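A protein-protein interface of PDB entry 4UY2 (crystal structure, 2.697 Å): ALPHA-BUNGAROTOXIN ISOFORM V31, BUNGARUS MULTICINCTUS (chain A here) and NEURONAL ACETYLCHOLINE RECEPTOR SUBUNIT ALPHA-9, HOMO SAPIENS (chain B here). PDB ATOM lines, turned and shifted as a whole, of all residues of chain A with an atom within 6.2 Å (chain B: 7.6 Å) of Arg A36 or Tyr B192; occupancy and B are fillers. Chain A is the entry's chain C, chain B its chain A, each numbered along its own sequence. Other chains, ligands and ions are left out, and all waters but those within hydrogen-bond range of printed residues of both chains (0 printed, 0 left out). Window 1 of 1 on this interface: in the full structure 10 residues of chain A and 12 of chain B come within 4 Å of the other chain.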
ATOM      1  N   ASP A  30      28.824 -18.974  27.300  1.00  0.00           N
ATOM      2  CA  ASP A  30      29.390 -17.674  27.000  1.00  0.00           C
ATOM      3  C   ASP A  30      29.296 -16.683  28.188  1.00  0.00           C
ATOM      4  O   ASP A  30      28.799 -17.039  29.260  1.00  0.00           O
ATOM      5  CB  ASP A  30      28.627 -17.184  25.776  1.00  0.00           C
ATOM      6  CG  ASP A  30      27.184 -16.854  26.098  1.00  0.00           C
ATOM      7  OD1 ASP A  30      26.822 -16.595  27.256  1.00  0.00           O
ATOM      8  OD2 ASP A  30      26.371 -17.004  25.174  1.00  0.00           O
ATOM      9  N   PHE A  32      27.995 -13.930  26.751  1.00  0.00           N
ATOM     10  CA  PHE A  32      26.983 -13.257  25.937  1.00  0.00           C
ATOM     11  C   PHE A  32      25.577 -13.623  26.462  1.00  0.00           C
ATOM     12  O   PHE A  32      24.579 -13.041  26.058  1.00  0.00           O
ATOM     13  CB  PHE A  32      27.076 -13.663  24.454  1.00  0.00           C
ATOM     14  CG  PHE A  32      27.891 -12.729  23.577  1.00  0.00           C
ATOM     15  CD1 PHE A  32      27.343 -11.518  23.143  1.00  0.00           C
ATOM     16  CD2 PHE A  32      29.158 -13.096  23.101  1.00  0.00           C
ATOM     17  CE1 PHE A  32      28.072 -10.642  22.321  1.00  0.00           C
ATOM     18  CE2 PHE A  32      29.897 -12.216  22.273  1.00  0.00           C
ATOM     19  CZ  PHE A  32      29.340 -11.005  21.882  1.00  0.00           C
ATOM     20  N   CYS A  33      25.539 -14.598  27.372  1.00  0.00           N
ATOM     21  CA  CYS A  33      24.333 -15.235  27.971  1.00  0.00           C
ATOM     22  C   CYS A  33      23.208 -14.275  28.327  1.00  0.00           C
ATOM     23  O   CYS A  33      22.045 -14.488  27.961  1.00  0.00           O
ATOM     24  CB  CYS A  33      24.763 -15.998  29.243  1.00  0.00           C
ATOM     25  SG  CYS A  33      24.018 -17.606  29.622  1.00  0.00           S
ATOM     26  N   SER A  34      23.576 -13.264  29.111  1.00  0.00           N
ATOM     27  CA  SER A  34      22.712 -12.152  29.436  1.00  0.00           C
ATOM     28  C   SER A  34      22.121 -11.525  28.161  1.00  0.00           C
ATOM     29  O   SER A  34      20.900 -11.391  28.039  1.00  0.00           O
ATOM     30  CB  SER A  34      23.517 -11.143  30.243  1.00  0.00           C
ATOM     31  OG  SER A  34      24.767 -10.940  29.601  1.00  0.00           O
ATOM     32  N   SER A  35      22.994 -11.216  27.195  1.00  0.00           N
ATOM     33  CA  SER A  35      22.660 -10.509  25.935  1.00  0.00           C
ATOM     34  C   SER A  35      21.943 -11.384  24.882  1.00  0.00           C
ATOM     35  O   SER A  35      20.989 -10.962  24.219  1.00  0.00           O
ATOM     36  CB  SER A  35      23.932  -9.952  25.308  1.00  0.00           C
ATOM     37  OG  SER A  35      24.941 -10.951  25.258  1.00  0.00           O
ATOM     38  N   ARG A  36      22.468 -12.578  24.672  1.00  0.00           N
ATOM     39  CA  ARG A  36      21.858 -13.511  23.747  1.00  0.00           C
ATOM     40  C   ARG A  36      21.935 -14.898  24.390  1.00  0.00           C
ATOM     41  O   ARG A  36      22.954 -15.578  24.364  1.00  0.00           O
ATOM     42  CB  ARG A  36      22.516 -13.452  22.354  1.00  0.00           C
ATOM     43  CG  ARG A  36      24.040 -13.371  22.236  1.00  0.00           C
ATOM     44  CD  ARG A  36      24.319 -12.810  20.844  1.00  0.00           C
ATOM     45  NE  ARG A  36      25.714 -12.745  20.419  1.00  0.00           N
ATOM     46  CZ  ARG A  36      26.101 -12.040  19.361  1.00  0.00           C
ATOM     47  NH1 ARG A  36      25.198 -11.367  18.662  1.00  0.00           N
ATOM     48  NH2 ARG A  36      27.372 -11.992  18.994  1.00  0.00           N
ATOM     49  N   GLY A  37      20.826 -15.293  24.988  1.00  0.00           N
ATOM     50  CA  GLY A  37      20.797 -16.436  25.868  1.00  0.00           C
ATOM     51  C   GLY A  37      21.440 -17.732  25.453  1.00  0.00           C
ATOM     52  O   GLY A  37      21.085 -18.293  24.425  1.00  0.00           O
ATOM     53  N   LYS A  38      22.443 -18.152  26.217  1.00  0.00           N
ATOM     54  CA  LYS A  38      22.828 -19.547  26.246  1.00  0.00           C
ATOM     55  C   LYS A  38      23.374 -20.139  24.920  1.00  0.00           C
ATOM     56  O   LYS A  38      22.736 -20.052  23.865  1.00  0.00           O
ATOM     57  CB  LYS A  38      21.576 -20.292  26.670  1.00  0.00           C
ATOM     58  CG  LYS A  38      21.799 -21.594  27.290  1.00  0.00           C
ATOM     59  CD  LYS A  38      22.412 -21.337  28.589  1.00  0.00           C
ATOM     60  CE  LYS A  38      23.008 -22.574  29.120  1.00  0.00           C
ATOM     61  NZ  LYS A  38      24.179 -22.084  29.818  1.00  0.00           N
ATOM     62  N   VAL A  39      24.516 -20.803  24.933  1.00  0.00           N
ATOM     63  CA  VAL A  39      24.976 -21.277  23.637  1.00  0.00           C
ATOM     64  C   VAL A  39      24.678 -22.717  23.528  1.00  0.00           C
ATOM     65  O   VAL A  39      24.999 -23.480  24.446  1.00  0.00           O
ATOM     66  CB  VAL A  39      26.491 -21.051  23.418  1.00  0.00           C
ATOM     67  CG1 VAL A  39      27.232 -21.259  24.705  1.00  0.00           C
ATOM     68  CG2 VAL A  39      27.049 -22.084  22.399  1.00  0.00           C
ATOM     69  N   VAL A  40      24.158 -23.074  22.342  1.00  0.00           N
ATOM     70  CA  VAL A  40      23.578 -24.387  22.018  1.00  0.00           C
ATOM     71  C   VAL A  40      24.349 -25.224  21.035  1.00  0.00           C
ATOM     72  O   VAL A  40      24.606 -24.793  19.931  1.00  0.00           O
ATOM     73  CB  VAL A  40      22.188 -24.243  21.387  1.00  0.00           C
ATOM     74  CG1 VAL A  40      21.587 -25.587  21.248  1.00  0.00           C
ATOM     75  CG2 VAL A  40      21.304 -23.377  22.221  1.00  0.00           C
ATOM     76  N   HIS A  68      16.710 -27.082  18.459  1.00  0.00           N
ATOM     77  CA  HIS A  68      17.084 -25.852  19.136  1.00  0.00           C
ATOM     78  C   HIS A  68      15.789 -25.277  19.729  1.00  0.00           C
ATOM     79  O   HIS A  68      14.696 -25.649  19.287  1.00  0.00           O
ATOM     80  CB  HIS A  68      17.786 -24.911  18.141  1.00  0.00           C
ATOM     81  CG  HIS A  68      18.301 -23.635  18.733  1.00  0.00           C
ATOM     82  ND1 HIS A  68      17.541 -22.487  18.835  1.00  0.00           N
ATOM     83  CD2 HIS A  68      19.502 -23.338  19.284  1.00  0.00           C
ATOM     84  CE1 HIS A  68      18.259 -21.539  19.404  1.00  0.00           C
ATOM     85  NE2 HIS A  68      19.454 -22.030  19.692  1.00  0.00           N
ATOM     86  N   VAL B  93      33.593  -7.201  16.532  1.00  0.00           N
ATOM     87  CA  VAL B  93      34.370  -7.100  17.763  1.00  0.00           C
ATOM     88  C   VAL B  93      35.240  -8.324  18.070  1.00  0.00           C
ATOM     89  O   VAL B  93      35.528  -9.069  17.163  1.00  0.00           O
ATOM     90  CB  VAL B  93      33.459  -6.819  18.901  1.00  0.00           C
ATOM     91  CG1 VAL B  93      32.347  -5.888  18.432  1.00  0.00           C
ATOM     92  CG2 VAL B  93      32.948  -8.115  19.476  1.00  0.00           C
ATOM     93  N   TYR B  95      35.265 -11.639  20.166  1.00  0.00           N
ATOM     94  CA  TYR B  95      34.498 -12.589  21.000  1.00  0.00           C
ATOM     95  C   TYR B  95      35.355 -13.208  22.076  1.00  0.00           C
ATOM     96  O   TYR B  95      34.912 -13.428  23.179  1.00  0.00           O
ATOM     97  CB  TYR B  95      33.923 -13.750  20.164  1.00  0.00           C
ATOM     98  CG  TYR B  95      32.578 -13.522  19.499  1.00  0.00           C
ATOM     99  CD1 TYR B  95      32.090 -12.227  19.287  1.00  0.00           C
ATOM    100  CD2 TYR B  95      31.819 -14.607  19.022  1.00  0.00           C
ATOM    101  CE1 TYR B  95      30.852 -12.007  18.655  1.00  0.00           C
ATOM    102  CE2 TYR B  95      30.574 -14.405  18.351  1.00  0.00           C
ATOM    103  CZ  TYR B  95      30.092 -13.092  18.191  1.00  0.00           C
ATOM    104  OH  TYR B  95      28.878 -12.838  17.553  1.00  0.00           O
ATOM    105  N   GLY B 149      33.720 -11.856  15.726  1.00  0.00           N
ATOM    106  CA  GLY B 149      32.437 -11.895  15.059  1.00  0.00           C
ATOM    107  C   GLY B 149      31.635 -10.668  15.378  1.00  0.00           C
ATOM    108  O   GLY B 149      31.917 -10.051  16.360  1.00  0.00           O
ATOM    109  N   SER B 150      30.532 -10.420  14.688  1.00  0.00           N
ATOM    110  CA  SER B 150      29.781  -9.204  14.909  1.00  0.00           C
ATOM    111  C   SER B 150      29.191  -9.084  16.266  1.00  0.00           C
ATOM    112  O   SER B 150      29.003 -10.072  16.971  1.00  0.00           O
ATOM    113  CB  SER B 150      28.653  -9.079  13.911  1.00  0.00           C
ATOM    114  OG  SER B 150      27.837  -7.976  14.297  1.00  0.00           O
ATOM    115  N   TRP B 151      28.885  -7.865  16.664  1.00  0.00           N
ATOM    116  CA  TRP B 151      28.357  -7.678  18.021  1.00  0.00           C
ATOM    117  C   TRP B 151      26.853  -7.635  17.994  1.00  0.00           C
ATOM    118  O   TRP B 151      26.210  -7.911  18.998  1.00  0.00           O
ATOM    119  CB  TRP B 151      28.934  -6.408  18.669  1.00  0.00           C
ATOM    120  CG  TRP B 151      28.431  -6.067  20.028  1.00  0.00           C
ATOM    121  CD1 TRP B 151      27.419  -5.204  20.342  1.00  0.00           C
ATOM    122  CD2 TRP B 151      28.944  -6.562  21.271  1.00  0.00           C
ATOM    123  NE1 TRP B 151      27.261  -5.139  21.710  1.00  0.00           N
ATOM    124  CE2 TRP B 151      28.179  -5.969  22.306  1.00  0.00           C
ATOM    125  CE3 TRP B 151      29.970  -7.459  21.613  1.00  0.00           C
ATOM    126  CZ2 TRP B 151      28.402  -6.257  23.672  1.00  0.00           C
ATOM    127  CZ3 TRP B 151      30.198  -7.745  22.975  1.00  0.00           C
ATOM    128  CH2 TRP B 151      29.408  -7.147  23.984  1.00  0.00           C
ATOM    129  N   THR B 152      26.285  -7.310  16.838  1.00  0.00           N
ATOM    130  CA  THR B 152      24.851  -7.070  16.780  1.00  0.00           C
ATOM    131  C   THR B 152      24.055  -7.763  15.647  1.00  0.00           C
ATOM    132  O   THR B 152      22.839  -7.565  15.565  1.00  0.00           O
ATOM    133  CB  THR B 152      24.585  -5.530  16.689  1.00  0.00           C
ATOM    134  OG1 THR B 152      24.939  -5.054  15.389  1.00  0.00           O
ATOM    135  CG2 THR B 152      25.404  -4.738  17.728  1.00  0.00           C
ATOM    136  N   TYR B 153      24.724  -8.567  14.803  1.00  0.00           N
ATOM    137  CA  TYR B 153      24.138  -9.109  13.558  1.00  0.00           C
ATOM    138  C   TYR B 153      24.419 -10.607  13.233  1.00  0.00           C
ATOM    139  O   TYR B 153      25.599 -10.982  13.028  1.00  0.00           O
ATOM    140  CB  TYR B 153      24.639  -8.285  12.346  1.00  0.00           C
ATOM    141  CG  TYR B 153      24.109  -6.869  12.240  1.00  0.00           C
ATOM    142  CD1 TYR B 153      22.791  -6.618  11.857  1.00  0.00           C
ATOM    143  CD2 TYR B 153      24.931  -5.791  12.466  1.00  0.00           C
ATOM    144  CE1 TYR B 153      22.299  -5.319  11.746  1.00  0.00           C
ATOM    145  CE2 TYR B 153      24.450  -4.493  12.358  1.00  0.00           C
ATOM    146  CZ  TYR B 153      23.133  -4.260  11.998  1.00  0.00           C
ATOM    147  OH  TYR B 153      22.661  -2.958  11.896  1.00  0.00           O
ATOM    148  N   ASN B 154      23.361 -11.438  13.133  1.00  0.00           N
ATOM    149  CA  ASN B 154      23.488 -12.837  12.636  1.00  0.00           C
ATOM    150  C   ASN B 154      24.050 -12.932  11.233  1.00  0.00           C
ATOM    151  O   ASN B 154      24.033 -11.952  10.478  1.00  0.00           O
ATOM    152  CB  ASN B 154      22.162 -13.574  12.645  1.00  0.00           C
ATOM    153  CG  ASN B 154      21.064 -12.753  12.056  1.00  0.00           C
ATOM    154  OD1 ASN B 154      21.109 -12.401  10.880  1.00  0.00           O
ATOM    155  ND2 ASN B 154      20.092 -12.386  12.874  1.00  0.00           N
ATOM    156  N   VAL B 189      30.028 -21.238  12.991  1.00  0.00           N
ATOM    157  CA  VAL B 189      28.813 -20.563  13.397  1.00  0.00           C
ATOM    158  C   VAL B 189      28.586 -20.916  14.814  1.00  0.00           C
ATOM    159  O   VAL B 189      29.013 -22.006  15.233  1.00  0.00           O
ATOM    160  CB  VAL B 189      27.582 -20.972  12.591  1.00  0.00           C
ATOM    161  CG1 VAL B 189      27.604 -20.308  11.240  1.00  0.00           C
ATOM    162  CG2 VAL B 189      27.470 -22.484  12.548  1.00  0.00           C
ATOM    163  N   ILE B 190      28.004 -19.959  15.546  1.00  0.00           N
ATOM    164  CA  ILE B 190      27.588 -20.176  16.920  1.00  0.00           C
ATOM    165  C   ILE B 190      26.087 -19.947  17.006  1.00  0.00           C
ATOM    166  O   ILE B 190      25.529 -18.915  16.594  1.00  0.00           O
ATOM    167  CB  ILE B 190      28.274 -19.251  17.922  1.00  0.00           C
ATOM    168  CG1 ILE B 190      29.717 -18.920  17.510  1.00  0.00           C
ATOM    169  CG2 ILE B 190      28.186 -19.876  19.314  1.00  0.00           C
ATOM    170  CD1 ILE B 190      30.695 -20.084  17.704  1.00  0.00           C
ATOM    171  N   SER B 191      25.458 -20.935  17.607  1.00  0.00           N
ATOM    172  CA  SER B 191      24.019 -21.097  17.661  1.00  0.00           C
ATOM    173  C   SER B 191      23.271 -20.115  18.577  1.00  0.00           C
ATOM    174  O   SER B 191      22.379 -19.404  18.098  1.00  0.00           O
ATOM    175  CB  SER B 191      23.803 -22.529  18.031  1.00  0.00           C
ATOM    176  OG  SER B 191      25.096 -23.003  18.438  1.00  0.00           O
ATOM    177  N   TYR B 192      23.592 -20.108  19.877  1.00  0.00           N
ATOM    178  CA  TYR B 192      23.004 -19.159  20.859  1.00  0.00           C
ATOM    179  C   TYR B 192      21.509 -19.289  21.085  1.00  0.00           C
ATOM    180  O   TYR B 192      20.696 -18.750  20.324  1.00  0.00           O
ATOM    181  CB  TYR B 192      23.311 -17.675  20.477  1.00  0.00           C
ATOM    182  CG  TYR B 192      24.739 -17.216  20.750  1.00  0.00           C
ATOM    183  CD1 TYR B 192      25.202 -17.131  22.041  1.00  0.00           C
ATOM    184  CD2 TYR B 192      25.618 -16.924  19.728  1.00  0.00           C
ATOM    185  CE1 TYR B 192      26.476 -16.752  22.313  1.00  0.00           C
ATOM    186  CE2 TYR B 192      26.884 -16.558  19.998  1.00  0.00           C
ATOM    187  CZ  TYR B 192      27.319 -16.471  21.291  1.00  0.00           C
ATOM    188  OH  TYR B 192      28.604 -16.077  21.600  1.00  0.00           O
ATOM    189  N   GLY B 193      21.153 -19.875  22.221  1.00  0.00           N
ATOM    190  CA  GLY B 193      19.778 -20.277  22.462  1.00  0.00           C
ATOM    191  C   GLY B 193      18.771 -19.147  22.461  1.00  0.00           C
ATOM    192  O   GLY B 193      17.571 -19.389  22.595  1.00  0.00           O
ATOM    193  N   CYS B 194      19.238 -17.917  22.289  1.00  0.00           N
ATOM    194  CA  CYS B 194      18.339 -16.783  22.453  1.00  0.00           C
ATOM    195  C   CYS B 194      17.358 -16.813  21.300  1.00  0.00           C
ATOM    196  O   CYS B 194      16.156 -16.617  21.468  1.00  0.00           O
ATOM    197  CB  CYS B 194      19.111 -15.454  22.443  1.00  0.00           C
ATOM    198  SG  CYS B 194      20.053 -15.257  20.931  1.00  0.00           S
ATOM    199  N   CYS B 195      17.915 -17.091  20.129  1.00  0.00           N
ATOM    200  CA  CYS B 195      17.207 -17.038  18.857  1.00  0.00           C
ATOM    201  C   CYS B 195      18.279 -17.464  17.833  1.00  0.00           C
ATOM    202  O   CYS B 195      18.852 -18.537  18.037  1.00  0.00           O
ATOM    203  CB  CYS B 195      16.585 -15.659  18.687  1.00  0.00           C
ATOM    204  SG  CYS B 195      17.691 -14.203  18.889  1.00  0.00           S
ATOM    205  N   SER B 196      18.586 -16.767  16.733  1.00  0.00           N
ATOM    206  CA  SER B 196      17.805 -16.279  15.583  1.00  0.00           C
ATOM    207  C   SER B 196      18.863 -16.434  14.532  1.00  0.00           C
ATOM    208  O   SER B 196      19.644 -15.505  14.336  1.00  0.00           O
ATOM    209  CB  SER B 196      17.348 -14.804  15.588  1.00  0.00           C
ATOM    210  OG  SER B 196      16.069 -14.565  16.140  1.00  0.00           O
ATOM    211  N   GLU B 197      18.974 -17.610  13.925  1.00  0.00           N
ATOM    212  CA  GLU B 197      19.995 -17.875  12.909  1.00  0.00           C
ATOM    213  C   GLU B 197      21.355 -18.015  13.627  1.00  0.00           C
ATOM    214  O   GLU B 197      21.495 -17.623  14.790  1.00  0.00           O
ATOM    215  CB  GLU B 197      20.040 -16.763  11.844  1.00  0.00           C
ATOM    216  CG  GLU B 197      18.703 -16.001  11.491  1.00  0.00           C
ATOM    217  CD  GLU B 197      17.379 -16.789  11.615  1.00  0.00           C
ATOM    218  OE1 GLU B 197      17.351 -18.044  11.545  1.00  0.00           O
ATOM    219  OE2 GLU B 197      16.344 -16.118  11.858  1.00  0.00           O
ATOM    220  N   PRO B 198      22.366 -18.590  12.968  1.00  0.00           N
ATOM    221  CA  PRO B 198      23.655 -18.616  13.671  1.00  0.00           C
ATOM    222  C   PRO B 198      24.506 -17.359  13.525  1.00  0.00           C
ATOM    223  O   PRO B 198      24.238 -16.435  12.736  1.00  0.00           O
ATOM    224  CB  PRO B 198      24.374 -19.820  13.053  1.00  0.00           C
ATOM    225  CG  PRO B 198      23.820 -19.960  11.724  1.00  0.00           C
ATOM    226  CD  PRO B 198      22.390 -19.429  11.760  1.00  0.00           C
ATOM    227  N   TYR B 199      25.535 -17.311  14.362  1.00  0.00           N
ATOM    228  CA  TYR B 199      26.421 -16.157  14.424  1.00  0.00           C
ATOM    229  C   TYR B 199      27.756 -16.635  13.884  1.00  0.00           C
ATOM    230  O   TYR B 199      28.415 -17.508  14.477  1.00  0.00           O
ATOM    231  CB  TYR B 199      26.519 -15.634  15.854  1.00  0.00           C
ATOM    232  CG  TYR B 199      25.324 -14.781  16.253  1.00  0.00           C
ATOM    233  CD1 TYR B 199      25.019 -13.630  15.549  1.00  0.00           C
ATOM    234  CD2 TYR B 199      24.496 -15.124  17.337  1.00  0.00           C
ATOM    235  CE1 TYR B 199      23.939 -12.838  15.891  1.00  0.00           C
ATOM    236  CE2 TYR B 199      23.413 -14.322  17.699  1.00  0.00           C
ATOM    237  CZ  TYR B 199      23.135 -13.177  16.954  1.00  0.00           C
ATOM    238  OH  TYR B 199      22.081 -12.324  17.240  1.00  0.00           O
ATOM    239  N   PRO B 200      28.132 -16.112  12.720  1.00  0.00           N
ATOM    240  CA  PRO B 200      29.371 -16.467  12.018  1.00  0.00           C
ATOM    241  C   PRO B 200      30.531 -15.911  12.786  1.00  0.00           C
ATOM    242  O   PRO B 200      30.409 -14.804  13.372  1.00  0.00           O
ATOM    243  CB  PRO B 200      29.230 -15.764  10.681  1.00  0.00           C
ATOM    244  CG  PRO B 200      28.416 -14.533  11.019  1.00  0.00           C
ATOM    245  CD  PRO B 200      27.400 -15.032  12.041  1.00  0.00           C
ATOM    246  N   ASP B 201      31.627 -16.660  12.831  1.00  0.00           N
ATOM    247  CA  ASP B 201      32.779 -16.139  13.539  1.00  0.00           C
ATOM    248  C   ASP B 201      34.051 -16.748  12.986  1.00  0.00           C
ATOM    249  O   ASP B 201      34.137 -17.989  12.859  1.00  0.00           O
ATOM    250  CB  ASP B 201      32.663 -16.408  15.054  1.00  0.00           C
ATOM    251  CG  ASP B 201      32.955 -17.818  15.416  1.00  0.00           C
ATOM    252  OD1 ASP B 201      32.065 -18.678  15.302  1.00  0.00           O
ATOM    253  OD2 ASP B 201      34.106 -18.072  15.791  1.00  0.00           O
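Of the printed residues of chain B, Asp A30 touches Tyr B192. Printed residues of chain B within 4 Å of Phe A32: Tyr B95, Trp B151 and Tyr B192. Arg A36 touches six residues of chain B. Gly A37 touches just these residues of chain B: Tyr B192 (3.5 Å), Gly B193 (2.7 Å) and Cys B194 (2.8 Å). Val B93 touches none of the printed residues of chain A. Of the printed residues of chain A, Ser B150 touches Arg A36 (3.2 Å). Printed residues of chain A within 4 Å of Trp B151: Phe A32 and Arg A36. Printed residues of chain A within 4 Å of Tyr B192: Asp A30 (2.9 Å), Phe A32 (3.4 Å), Arg A36 (3.6 Å), Gly A37 (3.5 Å), Lys A38 (3.1 Å), Val A40 (3.9 Å) and His A68 (3.6 Å). Of the printed residues of chain A, Gly B193 touches Gly A37 (2.7 Å), Lys A38 (2.3 Å), Val A40 (3.5 Å) and His A68 (3.3 Å). Pro B200 touches none of the printed residues of chain A. The nearest printed residue of chain A that does not touch Gly B193 is Val A39 (4.3 Å).
Hydrophobic or aromatic side chains of chain B that line the printed part of chain A: Tyr B95, Trp B151, Ile B190, Tyr B192 and Tyr B199. Along chain B the printed residues that touch a printed residue of chain A span positions 95 to 199. Of the 11 printed residues of chain A, 8 touch a printed residue of chain B. Among the printed residues, no Asp or Glu carboxylate lies within 4 Å of a Lys or Arg side-chain nitrogen of the other chain.
Among the printed residues, pairs that only touch across the chains: Asp A30 with Tyr B192 (2.9 Å), Phe A32 with Tyr B95 (3.7 Å), Phe A32 with Trp B151 (3.5 Å), Phe A32 with Tyr B192 (3.4 Å), Arg A36 with Trp B151 (3.6 Å), Arg A36 with Tyr B192 (3.6 Å), Arg A36 with Cys B194 (3.4 Å), Arg A36 with Tyr B199 (3.2 Å), Gly A37 with Tyr B192 (3.5 Å), Lys A38 with Tyr B192 (3.1 Å), Val A39 with Ile B190 (3.96 Å), Val A40 with Tyr B192 (3.9 Å), Val A40 with Gly B193 (3.5 Å), His A68 with Tyr B192 (3.6 Å), His A68 with Gly B193 (3.3 Å) and His A68 with Cys B195 (3.4 Å).
O of Ser B150 sits at hydrogen-bond distance from NH2 of Arg A36, at 3.2 Å. The backbone carbonyl oxygen (O) of Gly A37 sits at hydrogen-bond distance from the backbone NH (N) of Gly B193 (2.7 Å). O of Gly A37 is in hydrogen-bond range of N of Cys B194, at 2.8 Å. The side-chain hydroxyl (OH) of Tyr B95 lies close to the guanidinium group (NH2) of Arg A36 (2.2 Å). The backbone carbonyl oxygen (O) of Lys A38 lies close to the backbone NH (N) of Gly B193, 2.3 Å away. The backbone carbonyl oxygen of Val A40 lies close to the side-chain hydroxyl of Ser B191 (2.4 Å).
OH of Tyr B95 lies within hydrogen-bond range of O of Ser B150 (2.8 Å). O of Tyr B199 sits at hydrogen-bond distance from N of Ile B190 (2.7 Å). SG of Cys B194 is in hydrogen-bond range of O of Tyr B192, at 3.6 Å. The side-chain sulfur of Cys B195 sits close to the side-chain hydroxyl of Ser B196 (3.2 Å). OD1 of Asp A30 sits at hydrogen-bond distance from N of Phe A32, 3.0 Å away. The side-chain carboxylate of Asp A30 lies close to the backbone NH of Cys A33.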
